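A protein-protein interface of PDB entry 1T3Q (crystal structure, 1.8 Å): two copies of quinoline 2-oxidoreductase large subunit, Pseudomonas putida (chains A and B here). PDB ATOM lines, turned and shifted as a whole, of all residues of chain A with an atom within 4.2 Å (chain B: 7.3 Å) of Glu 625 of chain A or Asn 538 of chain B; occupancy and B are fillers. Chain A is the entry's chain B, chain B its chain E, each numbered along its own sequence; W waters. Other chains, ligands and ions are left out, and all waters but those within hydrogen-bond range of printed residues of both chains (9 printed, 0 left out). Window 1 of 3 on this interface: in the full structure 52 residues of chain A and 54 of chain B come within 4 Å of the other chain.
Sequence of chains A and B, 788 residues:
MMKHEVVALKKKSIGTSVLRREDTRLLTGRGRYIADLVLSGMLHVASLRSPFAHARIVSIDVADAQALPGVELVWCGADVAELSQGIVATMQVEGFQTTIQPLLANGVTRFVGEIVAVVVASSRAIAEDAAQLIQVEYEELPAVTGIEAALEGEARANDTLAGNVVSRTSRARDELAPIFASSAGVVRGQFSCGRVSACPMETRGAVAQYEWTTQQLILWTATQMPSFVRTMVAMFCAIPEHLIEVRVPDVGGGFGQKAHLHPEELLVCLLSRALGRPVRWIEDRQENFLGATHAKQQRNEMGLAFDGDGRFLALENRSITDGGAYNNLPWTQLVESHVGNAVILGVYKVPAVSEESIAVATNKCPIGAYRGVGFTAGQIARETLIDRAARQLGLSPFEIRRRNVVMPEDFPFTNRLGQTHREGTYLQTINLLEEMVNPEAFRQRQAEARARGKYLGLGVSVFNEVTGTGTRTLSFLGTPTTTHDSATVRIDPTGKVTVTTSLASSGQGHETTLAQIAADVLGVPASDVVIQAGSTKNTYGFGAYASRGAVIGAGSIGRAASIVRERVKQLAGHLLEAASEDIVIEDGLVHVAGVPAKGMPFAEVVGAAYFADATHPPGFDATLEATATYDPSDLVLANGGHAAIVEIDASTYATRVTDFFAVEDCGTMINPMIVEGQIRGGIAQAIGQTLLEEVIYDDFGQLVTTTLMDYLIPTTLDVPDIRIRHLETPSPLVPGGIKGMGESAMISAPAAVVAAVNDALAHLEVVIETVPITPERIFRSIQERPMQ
NH1 of Arg 490 of chain A lies within hydrogen-bond range of O of Thr 539 of chain B (2.9 Å).
The guanidinium group of Arg 490 of chain A lies within hydrogen-bond range of the backbone carbonyl oxygen of Thr 536 of chain B (2.8 Å).
ND2 of Asn 538 of chain B sits at hydrogen-bond distance from OE1 of Glu 625 of chain A (3.3 Å).
The side-chain hydroxyl (OG1) of Thr 500 of chain A sits at hydrogen-bond distance from the side-chain amide nitrogen (ND2) of Asn 538 of chain B (3.3 Å).
OG1 of Thr 500 of chain B sits at hydrogen-bond distance from ND2 of Asn 538 of chain A, at 3.3 Å.
ND2 of Asn 538 of chain A lies within hydrogen-bond range of OE1 of Glu 625 of chain B, at 3.4 Å.
The side-chain carboxylate (OE2) of Glu 625 of chain A sits at hydrogen-bond distance from the backbone NH (N) of Thr 539 of chain B, at 2.8 Å.
The side-chain amide nitrogen of Gln 532 of chain A sits at hydrogen-bond distance from the backbone carbonyl oxygen of Lys 537 of chain B (3.3 Å).
The side-chain hydroxyl of Thr 623 of chain A sits at hydrogen-bond distance from the backbone NH of Thr 629 of chain B (2.9 Å).
OD1 of Asn 538 of chain A lies close to OD1 of Asn 538 of chain B.
The guanidinium group (NH1) of Arg 490 of chain A sits at hydrogen-bond distance from the backbone carbonyl oxygen (O) of Lys 537 of chain B (3.5 Å).
Thr 500 of chain A touches Asn 538 of chain B, and with the chains exchanged Asn 538 of chain A touches Thr 500 of chain B.
Asn 538 of chain A touches Thr 488 of chain B, but with the chains exchanged Thr 488 of chain A does not touch Asn 538 of chain B (4.1 Å).
Asn 538 of chain B touches its own counterpart, Asn 538 of chain A.
Asn 538 of chain A touches Glu 625 of chain B, and with the chains exchanged Glu 625 of chain A touches Asn 538 of chain B.
Along chain A the printed residues that touch a printed residue of chain B span positions 490 to 625.
Along chain B the printed residues that touch a printed residue of chain A span positions 488 to 629.
Among the printed residues, 16 pairs touch across the chains.
Among the printed residues, no Asp or Glu carboxylate lies within 4 Å of a Lys or Arg side-chain nitrogen of the other chain.
Glu 625 of chain A touches just these residues of chain B: Asn 538 (3.3 Å), Thr 539 (2.8 Å) and Thr 627 (3.5 Å).
Asn 538 of chain B touches just these residues of chain A: Arg 490 (3.5 Å), Thr 500 (3.3 Å), Asn 538 (3.3 Å) and Glu 625 (3.3 Å).
Of the printed residues of chain B, Gln 532 of chain A touches Lys 537 (3.3 Å).
Of the printed residues of chain A, Thr 536 of chain B touches Arg 490 (2.8 Å).
Printed residues of chain A within 4 Å of Lys 537 of chain B: Arg 490 and Gln 532.
Of the printed residues of chain A, Glu 625 of chain B touches Asn 538.
Thr 501 of chain B touches none of the printed residues of chain A.
The nearest residue of chain B that does not touch Glu 625 of chain A is Ser 486 of chain B (4.3 Å).
The nearest printed residue of chain A that does not touch Thr 488 of chain B is Glu 625 of chain A (4.7 Å).
Among the printed residues, merely in contact across the chains: Arg 490 of chain A with Asn 538 of chain B, Asn 538 of chain A with Thr 488 of chain B, Thr 623 of chain A with Thr 627 of chain B, Thr 623 of chain A with Ala 628 of chain B and Glu 625 of chain A with Thr 627 of chain B.
OG1 of Thr 500 of chain B is in hydrogen-bond range of NE2 of Gln 532 of chain B, 3.0 Å away.
O of Thr 488 of chain A lies within hydrogen-bond range of N of Thr 500 of chain A.
O of Ala 628 of chain B sits at hydrogen-bond distance from N of Ala 487 of chain B.
OG of Ser 502 of chain B is in hydrogen-bond range of OG1 of Thr 539 of chain B, 2.6 Å away.
The backbone NH (N) of Lys 537 of chain B sits close to the side-chain hydroxyl (OG) of Ser 535 of chain B (3.3 Å).
NE2 of Gln 532 of chain A lies within hydrogen-bond range of OG1 of Thr 500 of chain A (3.0 Å).
Water W8 lies within hydrogen-bond range of OE1 of Glu 625 of chain A, OG1 of Thr 488 of chain B and OG1 of Thr 627 of chain B.
Water W4 lies within hydrogen-bond range of the side-chain hydroxyl (OG) of Ser 486 of chain B, the side-chain carboxylate (OE2) of Glu 625 of chain A and the backbone NH (N) of Tyr 540 of chain B.
Water W1 lies within hydrogen-bond range of O of Glu 625 of chain A and O of Thr 627 of chain B.
Water W6 bridges OE1 of Glu 625 of chain B (2.8 Å) and ND2 of Asn 538 of chain A (3.4 Å).
Water W9 bridges the side-chain amide oxygen of Asn 538 of chain B (2.9 Å) and the side-chain amide oxygen of Asn 538 of chain A (3.4 Å).
Water W2 bridges the backbone NH (N) of Leu 624 of chain A (3.0 Å) and a ring nitrogen (NE2) of His 484 of chain B (3.3 Å).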
ATOM      1  N   THR A 488     -17.503  16.729  18.436  1.00  0.00           N
ATOM      2  CA  THR A 488     -17.344  17.056  19.833  1.00  0.00           C
ATOM      3  C   THR A 488     -18.729  17.049  20.446  1.00  0.00           C
ATOM      4  O   THR A 488     -19.701  17.461  19.810  1.00  0.00           O
ATOM      5  CB  THR A 488     -16.693  18.440  20.028  1.00  0.00           C
ATOM      6  OG1 THR A 488     -15.362  18.418  19.493  1.00  0.00           O
ATOM      7  CG2 THR A 488     -16.629  18.796  21.502  1.00  0.00           C
ATOM      8  N   VAL A 489     -18.814  16.545  21.668  1.00  0.00           N
ATOM      9  CA  VAL A 489     -20.077  16.489  22.378  1.00  0.00           C
ATOM     10  C   VAL A 489     -19.843  16.967  23.794  1.00  0.00           C
ATOM     11  O   VAL A 489     -18.933  16.492  24.481  1.00  0.00           O
ATOM     12  CB  VAL A 489     -20.650  15.050  22.417  1.00  0.00           C
ATOM     13  CG1 VAL A 489     -21.891  15.008  23.302  1.00  0.00           C
ATOM     14  CG2 VAL A 489     -21.006  14.596  21.015  1.00  0.00           C
ATOM     15  N   ARG A 490     -20.653  17.928  24.217  1.00  0.00           N
ATOM     16  CA  ARG A 490     -20.570  18.465  25.561  1.00  0.00           C
ATOM     17  C   ARG A 490     -21.931  18.335  26.205  1.00  0.00           C
ATOM     18  O   ARG A 490     -22.948  18.635  25.585  1.00  0.00           O
ATOM     19  CB  ARG A 490     -20.195  19.954  25.548  1.00  0.00           C
ATOM     20  CG  ARG A 490     -20.263  20.612  26.932  1.00  0.00           C
ATOM     21  CD  ARG A 490     -19.906  22.098  26.864  1.00  0.00           C
ATOM     22  NE  ARG A 490     -20.936  22.869  26.171  1.00  0.00           N
ATOM     23  CZ  ARG A 490     -20.741  24.068  25.629  1.00  0.00           C
ATOM     24  NH1 ARG A 490     -19.548  24.648  25.694  1.00  0.00           N
ATOM     25  NH2 ARG A 490     -21.737  24.684  25.011  1.00  0.00           N
ATOM     26  N   THR A 500     -20.852  19.435  18.234  1.00  0.00           N
ATOM     27  CA  THR A 500     -20.137  20.217  17.236  1.00  0.00           C
ATOM     28  C   THR A 500     -19.663  19.241  16.170  1.00  0.00           C
ATOM     29  O   THR A 500     -19.033  18.223  16.469  1.00  0.00           O
ATOM     30  CB  THR A 500     -18.924  20.961  17.831  1.00  0.00           C
ATOM     31  OG1 THR A 500     -19.355  21.784  18.923  1.00  0.00           O
ATOM     32  CG2 THR A 500     -18.280  21.859  16.770  1.00  0.00           C
ATOM     33  N   GLN A 532     -24.080  22.129  16.271  1.00  0.00           N
ATOM     34  CA  GLN A 532     -23.254  23.270  15.894  1.00  0.00           C
ATOM     35  C   GLN A 532     -22.399  22.852  14.711  1.00  0.00           C
ATOM     36  O   GLN A 532     -21.668  21.865  14.786  1.00  0.00           O
ATOM     37  CB  GLN A 532     -22.347  23.685  17.059  1.00  0.00           C
ATOM     38  CG  GLN A 532     -23.096  24.297  18.218  1.00  0.00           C
ATOM     39  CD  GLN A 532     -22.185  24.787  19.318  1.00  0.00           C
ATOM     40  OE1 GLN A 532     -22.551  25.678  20.077  1.00  0.00           O
ATOM     41  NE2 GLN A 532     -20.995  24.201  19.422  1.00  0.00           N
ATOM     42  N   ASN A 538     -13.524  24.338  15.938  1.00  0.00           N
ATOM     43  CA  ASN A 538     -13.457  23.076  16.672  1.00  0.00           C
ATOM     44  C   ASN A 538     -13.905  21.920  15.785  1.00  0.00           C
ATOM     45  O   ASN A 538     -14.792  22.074  14.942  1.00  0.00           O
ATOM     46  CB  ASN A 538     -14.312  23.144  17.945  1.00  0.00           C
ATOM     47  CG  ASN A 538     -13.801  24.186  18.937  1.00  0.00           C
ATOM     48  OD1 ASN A 538     -14.134  25.373  18.846  1.00  0.00           O
ATOM     49  ND2 ASN A 538     -12.971  23.747  19.874  1.00  0.00           N
ATOM     50  N   VAL A 564     -18.329  10.864  27.080  1.00  0.00           N
ATOM     51  CA  VAL A 564     -18.943  11.590  28.178  1.00  0.00           C
ATOM     52  C   VAL A 564     -20.056  10.769  28.827  1.00  0.00           C
ATOM     53  O   VAL A 564     -20.287  10.876  30.032  1.00  0.00           O
ATOM     54  CB  VAL A 564     -19.461  12.974  27.716  1.00  0.00           C
ATOM     55  CG1 VAL A 564     -18.280  13.829  27.286  1.00  0.00           C
ATOM     56  CG2 VAL A 564     -20.449  12.827  26.572  1.00  0.00           C
ATOM     57  N   THR A 623     -14.511  15.832  33.272  1.00  0.00           N
ATOM     58  CA  THR A 623     -14.678  16.510  31.991  1.00  0.00           C
ATOM     59  C   THR A 623     -15.879  15.949  31.231  1.00  0.00           C
ATOM     60  O   THR A 623     -15.888  14.768  30.874  1.00  0.00           O
ATOM     61  CB  THR A 623     -13.440  16.335  31.096  1.00  0.00           C
ATOM     62  OG1 THR A 623     -12.257  16.649  31.843  1.00  0.00           O
ATOM     63  CG2 THR A 623     -13.532  17.263  29.893  1.00  0.00           C
ATOM     64  N   LEU A 624     -16.888  16.783  30.977  1.00  0.00           N
ATOM     65  CA  LEU A 624     -18.060  16.313  30.243  1.00  0.00           C
ATOM     66  C   LEU A 624     -18.167  16.832  28.808  1.00  0.00           C
ATOM     67  O   LEU A 624     -19.260  17.080  28.300  1.00  0.00           O
ATOM     68  CB  LEU A 624     -19.354  16.614  31.017  1.00  0.00           C
ATOM     69  CG  LEU A 624     -19.629  15.732  32.246  1.00  0.00           C
ATOM     70  CD1 LEU A 624     -21.066  15.955  32.715  1.00  0.00           C
ATOM     71  CD2 LEU A 624     -19.427  14.254  31.908  1.00  0.00           C
ATOM     72  N   GLU A 625     -17.016  16.993  28.163  1.00  0.00           N
ATOM     73  CA  GLU A 625     -16.946  17.416  26.771  1.00  0.00           C
ATOM     74  C   GLU A 625     -15.810  16.590  26.184  1.00  0.00           C
ATOM     75  O   GLU A 625     -14.718  16.535  26.755  1.00  0.00           O
ATOM     76  CB  GLU A 625     -16.632  18.917  26.647  1.00  0.00           C
ATOM     77  CG  GLU A 625     -16.605  19.405  25.197  1.00  0.00           C
ATOM     78  CD  GLU A 625     -16.617  20.927  25.069  1.00  0.00           C
ATOM     79  OE1 GLU A 625     -16.628  21.422  23.922  1.00  0.00           O
ATOM     80  OE2 GLU A 625     -16.622  21.624  26.107  1.00  0.00           O
ATOM     81  N   ALA A 626     -16.069  15.933  25.060  1.00  0.00           N
ATOM     82  CA  ALA A 626     -15.053  15.092  24.440  1.00  0.00           C
ATOM     83  C   ALA A 626     -15.134  15.127  22.925  1.00  0.00           C
ATOM     84  O   ALA A 626     -16.177  15.449  22.351  1.00  0.00           O
ATOM     85  CB  ALA A 626     -15.200  13.649  24.938  1.00  0.00           C
ATOM     86  N   SER B 227     -19.137  31.420  30.877  1.00  0.00           N
ATOM     87  CA  SER B 227     -19.904  30.189  31.102  1.00  0.00           C
ATOM     88  C   SER B 227     -20.917  30.364  32.233  1.00  0.00           C
ATOM     89  O   SER B 227     -22.044  29.862  32.165  1.00  0.00           O
ATOM     90  CB  SER B 227     -18.969  29.022  31.440  1.00  0.00           C
ATOM     91  OG  SER B 227     -18.077  28.755  30.372  1.00  0.00           O
ATOM     92  N   GLU B 245     -25.761  31.293  23.785  1.00  0.00           N
ATOM     93  CA  GLU B 245     -24.333  31.442  23.579  1.00  0.00           C
ATOM     94  C   GLU B 245     -23.932  32.804  24.125  1.00  0.00           C
ATOM     95  O   GLU B 245     -24.561  33.820  23.814  1.00  0.00           O
ATOM     96  CB  GLU B 245     -23.935  31.373  22.100  1.00  0.00           C
ATOM     97  CG  GLU B 245     -22.420  31.617  21.927  1.00  0.00           C
ATOM     98  CD  GLU B 245     -21.969  31.787  20.481  1.00  0.00           C
ATOM     99  OE1 GLU B 245     -20.750  31.985  20.257  1.00  0.00           O
ATOM    100  OE2 GLU B 245     -22.816  31.728  19.568  1.00  0.00           O
ATOM    101  N   HIS B 484     -15.310  24.080  37.793  1.00  0.00           N
ATOM    102  CA  HIS B 484     -15.143  23.291  36.577  1.00  0.00           C
ATOM    103  C   HIS B 484     -14.488  24.233  35.579  1.00  0.00           C
ATOM    104  O   HIS B 484     -14.984  25.330  35.341  1.00  0.00           O
ATOM    105  CB  HIS B 484     -16.503  22.822  36.051  1.00  0.00           C
ATOM    106  CG  HIS B 484     -16.412  21.732  35.027  1.00  0.00           C
ATOM    107  ND1 HIS B 484     -16.116  21.973  33.702  1.00  0.00           N
ATOM    108  CD2 HIS B 484     -16.562  20.391  35.142  1.00  0.00           C
ATOM    109  CE1 HIS B 484     -16.088  20.826  33.044  1.00  0.00           C
ATOM    110  NE2 HIS B 484     -16.357  19.851  33.895  1.00  0.00           N
ATOM    111  N   SER B 486     -12.597  23.651  31.864  1.00  0.00           N
ATOM    112  CA  SER B 486     -12.004  22.849  30.811  1.00  0.00           C
ATOM    113  C   SER B 486     -11.336  23.707  29.751  1.00  0.00           C
ATOM    114  O   SER B 486     -11.593  24.908  29.635  1.00  0.00           O
ATOM    115  CB  SER B 486     -13.067  21.961  30.155  1.00  0.00           C
ATOM    116  OG  SER B 486     -13.967  22.723  29.365  1.00  0.00           O
ATOM    117  N   ALA B 487     -10.453  23.068  28.997  1.00  0.00           N
ATOM    118  CA  ALA B 487      -9.742  23.700  27.900  1.00  0.00           C
ATOM    119  C   ALA B 487      -9.715  22.658  26.796  1.00  0.00           C
ATOM    120  O   ALA B 487      -9.755  21.454  27.069  1.00  0.00           O
ATOM    121  CB  ALA B 487      -8.322  24.059  28.314  1.00  0.00           C
ATOM    122  N   THR B 488      -9.660  23.115  25.553  1.00  0.00           N
ATOM    123  CA  THR B 488      -9.607  22.218  24.412  1.00  0.00           C
ATOM    124  C   THR B 488      -8.345  22.537  23.622  1.00  0.00           C
ATOM    125  O   THR B 488      -7.991  23.698  23.443  1.00  0.00           O
ATOM    126  CB  THR B 488     -10.835  22.393  23.495  1.00  0.00           C
ATOM    127  OG1 THR B 488     -12.014  21.965  24.192  1.00  0.00           O
ATOM    128  CG2 THR B 488     -10.684  21.576  22.217  1.00  0.00           C
ATOM    129  N   THR B 500      -8.670  26.384  22.850  1.00  0.00           N
ATOM    130  CA  THR B 500      -9.929  27.021  23.217  1.00  0.00           C
ATOM    131  C   THR B 500     -10.013  26.994  24.743  1.00  0.00           C
ATOM    132  O   THR B 500      -9.759  25.960  25.366  1.00  0.00           O
ATOM    133  CB  THR B 500     -11.154  26.281  22.649  1.00  0.00           C
ATOM    134  OG1 THR B 500     -10.972  26.040  21.248  1.00  0.00           O
ATOM    135  CG2 THR B 500     -12.419  27.130  22.852  1.00  0.00           C
ATOM    136  N   THR B 501     -10.368  28.130  25.336  1.00  0.00           N
ATOM    137  CA  THR B 501     -10.475  28.257  26.792  1.00  0.00           C
ATOM    138  C   THR B 501     -11.745  29.027  27.158  1.00  0.00           C
ATOM    139  O   THR B 501     -12.285  29.767  26.333  1.00  0.00           O
ATOM    140  CB  THR B 501      -9.247  29.025  27.369  1.00  0.00           C
ATOM    141  OG1 THR B 501      -9.362  29.143  28.796  1.00  0.00           O
ATOM    142  CG2 THR B 501      -9.167  30.427  26.765  1.00  0.00           C
ATOM    143  N   SER B 502     -12.226  28.840  28.385  1.00  0.00           N
ATOM    144  CA  SER B 502     -13.411  29.563  28.842  1.00  0.00           C
ATOM    145  C   SER B 502     -12.969  30.703  29.748  1.00  0.00           C
ATOM    146  O   SER B 502     -13.786  31.368  30.384  1.00  0.00           O
ATOM    147  CB  SER B 502     -14.382  28.638  29.584  1.00  0.00           C
ATOM    148  OG  SER B 502     -15.209  27.946  28.664  1.00  0.00           O
ATOM    149  N   GLN B 532      -8.190  30.727  21.540  1.00  0.00           N
ATOM    150  CA  GLN B 532      -9.567  31.074  21.207  1.00  0.00           C
ATOM    151  C   GLN B 532     -10.357  31.202  22.496  1.00  0.00           C
ATOM    152  O   GLN B 532     -10.442  30.257  23.274  1.00  0.00           O
ATOM    153  CB  GLN B 532     -10.207  29.984  20.339  1.00  0.00           C
ATOM    154  CG  GLN B 532      -9.622  29.870  18.956  1.00  0.00           C
ATOM    155  CD  GLN B 532     -10.296  28.808  18.110  1.00  0.00           C
ATOM    156  OE1 GLN B 532     -10.309  28.908  16.889  1.00  0.00           O
ATOM    157  NE2 GLN B 532     -10.845  27.775  18.751  1.00  0.00           N
ATOM    158  N   SER B 535     -16.244  32.733  23.736  1.00  0.00           N
ATOM    159  CA  SER B 535     -17.406  32.035  23.197  1.00  0.00           C
ATOM    160  C   SER B 535     -17.690  30.775  24.001  1.00  0.00           C
ATOM    161  O   SER B 535     -16.781  30.000  24.276  1.00  0.00           O
ATOM    162  CB  SER B 535     -17.178  31.655  21.737  1.00  0.00           C
ATOM    163  OG  SER B 535     -18.232  30.824  21.281  1.00  0.00           O
ATOM    164  N   THR B 536     -18.953  30.575  24.371  1.00  0.00           N
ATOM    165  CA  THR B 536     -19.340  29.396  25.140  1.00  0.00           C
ATOM    166  C   THR B 536     -19.695  28.196  24.265  1.00  0.00           C
ATOM    167  O   THR B 536     -20.227  27.197  24.763  1.00  0.00           O
ATOM    168  CB  THR B 536     -20.553  29.707  26.055  1.00  0.00           C
ATOM    169  OG1 THR B 536     -21.619  30.237  25.261  1.00  0.00           O
ATOM    170  CG2 THR B 536     -20.174  30.720  27.131  1.00  0.00           C
ATOM    171  N   LYS B 537     -19.399  28.278  22.969  1.00  0.00           N
ATOM    172  CA  LYS B 537     -19.707  27.176  22.070  1.00  0.00           C
ATOM    173  C   LYS B 537     -18.951  25.904  22.440  1.00  0.00           C
ATOM    174  O   LYS B 537     -19.451  24.803  22.226  1.00  0.00           O
ATOM    175  CB  LYS B 537     -19.385  27.549  20.621  1.00  0.00           C
ATOM    176  CG  LYS B 537     -20.475  28.355  19.923  1.00  0.00           C
ATOM    177  CD  LYS B 537     -20.187  28.421  18.429  1.00  0.00           C
ATOM    178  CE  LYS B 537     -21.352  28.994  17.649  1.00  0.00           C
ATOM    179  NZ  LYS B 537     -21.076  28.932  16.187  1.00  0.00           N
ATOM    180  N   ASN B 538     -17.747  26.067  22.984  1.00  0.00           N
ATOM    181  CA  ASN B 538     -16.913  24.940  23.389  1.00  0.00           C
ATOM    182  C   ASN B 538     -16.128  25.275  24.656  1.00  0.00           C
ATOM    183  O   ASN B 538     -15.681  26.410  24.838  1.00  0.00           O
ATOM    184  CB  ASN B 538     -15.969  24.539  22.248  1.00  0.00           C
ATOM    185  CG  ASN B 538     -16.721  24.091  21.002  1.00  0.00           C
ATOM    186  OD1 ASN B 538     -17.102  24.907  20.168  1.00  0.00           O
ATOM    187  ND2 ASN B 538     -16.958  22.788  20.887  1.00  0.00           N
ATOM    188  N   THR B 539     -15.966  24.262  25.509  1.00  0.00           N
ATOM    189  CA  THR B 539     -15.305  24.334  26.822  1.00  0.00           C
ATOM    190  C   THR B 539     -16.283  24.945  27.821  1.00  0.00           C
ATOM    191  O   THR B 539     -17.346  25.427  27.440  1.00  0.00           O
ATOM    192  CB  THR B 539     -13.969  25.159  26.843  1.00  0.00           C
ATOM    193  OG1 THR B 539     -14.236  26.555  26.668  1.00  0.00           O
ATOM    194  CG2 THR B 539     -13.018  24.671  25.762  1.00  0.00           C
ATOM    195  N   TYR B 540     -15.932  24.899  29.102  1.00  0.00           N
ATOM    196  CA  TYR B 540     -16.785  25.444  30.153  1.00  0.00           C
ATOM    197  C   TYR B 540     -15.901  25.734  31.352  1.00  0.00           C
ATOM    198  O   TYR B 540     -15.143  24.872  31.793  1.00  0.00           O
ATOM    199  CB  TYR B 540     -17.875  24.431  30.534  1.00  0.00           C
ATOM    200  CG  TYR B 540     -18.901  24.971  31.511  1.00  0.00           C
ATOM    201  CD1 TYR B 540     -18.590  25.142  32.861  1.00  0.00           C
ATOM    202  CD2 TYR B 540     -20.164  25.362  31.072  1.00  0.00           C
ATOM    203  CE1 TYR B 540     -19.519  25.698  33.750  1.00  0.00           C
ATOM    204  CE2 TYR B 540     -21.093  25.917  31.945  1.00  0.00           C
ATOM    205  CZ  TYR B 540     -20.765  26.084  33.278  1.00  0.00           C
ATOM    206  OH  TYR B 540     -21.681  26.657  34.133  1.00  0.00           O
ATOM    207  N   GLY B 541     -15.985  26.952  31.874  1.00  0.00           N
ATOM    208  CA  GLY B 541     -15.160  27.309  33.011  1.00  0.00           C
ATOM    209  C   GLY B 541     -15.727  28.458  33.807  1.00  0.00           C
ATOM    210  O   GLY B 541     -16.595  29.183  33.328  1.00  0.00           O
ATOM    211  N   GLU B 625      -7.538  16.238  18.952  1.00  0.00           N
ATOM    212  CA  GLU B 625      -8.226  17.352  19.585  1.00  0.00           C
ATOM    213  C   GLU B 625      -8.828  16.738  20.841  1.00  0.00           C
ATOM    214  O   GLU B 625      -9.528  15.722  20.766  1.00  0.00           O
ATOM    215  CB  GLU B 625      -9.331  17.924  18.686  1.00  0.00           C
ATOM    216  CG  GLU B 625     -10.080  19.104  19.327  1.00  0.00           C
ATOM    217  CD  GLU B 625     -10.942  19.895  18.340  1.00  0.00           C
ATOM    218  OE1 GLU B 625     -11.522  20.929  18.746  1.00  0.00           O
ATOM    219  OE2 GLU B 625     -11.038  19.492  17.163  1.00  0.00           O
ATOM    220  N   ALA B 626      -8.542  17.331  21.994  1.00  0.00           N
ATOM    221  CA  ALA B 626      -9.048  16.804  23.256  1.00  0.00           C
ATOM    222  C   ALA B 626      -9.420  17.917  24.224  1.00  0.00           C
ATOM    223  O   ALA B 626      -8.945  19.046  24.104  1.00  0.00           O
ATOM    224  CB  ALA B 626      -8.009  15.890  23.888  1.00  0.00           C
ATOM    225  N   THR B 627     -10.271  17.573  25.187  1.00  0.00           N
ATOM    226  CA  THR B 627     -10.750  18.516  26.190  1.00  0.00           C
ATOM    227  C   THR B 627     -10.572  17.942  27.594  1.00  0.00           C
ATOM    228  O   THR B 627     -10.766  16.744  27.820  1.00  0.00           O
ATOM    229  CB  THR B 627     -12.253  18.836  25.954  1.00  0.00           C
ATOM    230  OG1 THR B 627     -12.412  19.448  24.668  1.00  0.00           O
ATOM    231  CG2 THR B 627     -12.791  19.771  27.026  1.00  0.00           C
ATOM    232  N   ALA B 628     -10.191  18.794  28.536  1.00  0.00           N
ATOM    233  CA  ALA B 628     -10.003  18.356  29.913  1.00  0.00           C
ATOM    234  C   ALA B 628     -10.206  19.486  30.908  1.00  0.00           C
ATOM    235  O   ALA B 628      -9.839  20.637  30.646  1.00  0.00           O
ATOM    236  CB  ALA B 628      -8.602  17.752  30.089  1.00  0.00           C
ATOM    237  N   THR B 629     -10.805  19.153  32.047  1.00  0.00           N
ATOM    238  CA  THR B 629     -11.016  20.131  33.096  1.00  0.00           C
ATOM    239  C   THR B 629      -9.870  19.966  34.087  1.00  0.00           C
ATOM    240  O   THR B 629      -9.295  18.878  34.208  1.00  0.00           O
ATOM    241  CB  THR B 629     -12.364  19.919  33.826  1.00  0.00           C
ATOM    242  OG1 THR B 629     -12.589  21.009  34.730  1.00  0.00           O
ATOM    243  CG2 THR B 629     -12.362  18.613  34.606  1.00  0.00           C
HETATM  244  O   HOH W   1     -12.770  14.782  27.236  1.00  0.00           O
HETATM  245  O   HOH W   2     -17.281  19.712  30.722  1.00  0.00           O
HETATM  246  O   HOH W   3     -19.298  22.208  23.151  1.00  0.00           O
HETATM  247  O   HOH W   4     -16.154  21.449  28.808  1.00  0.00           O
HETATM  248  O   HOH W   5     -13.709  20.443  20.219  1.00  0.00           O
HETATM  249  O   HOH W   6     -10.118  23.304  18.120  1.00  0.00           O
HETATM  250  O   HOH W   7     -15.149  27.539  19.823  1.00  0.00           O
HETATM  251  O   HOH W   8     -14.322  21.373  22.796  1.00  0.00           O
HETATM  252  O   HOH W   9     -17.181  25.747  17.364  1.00  0.00           O
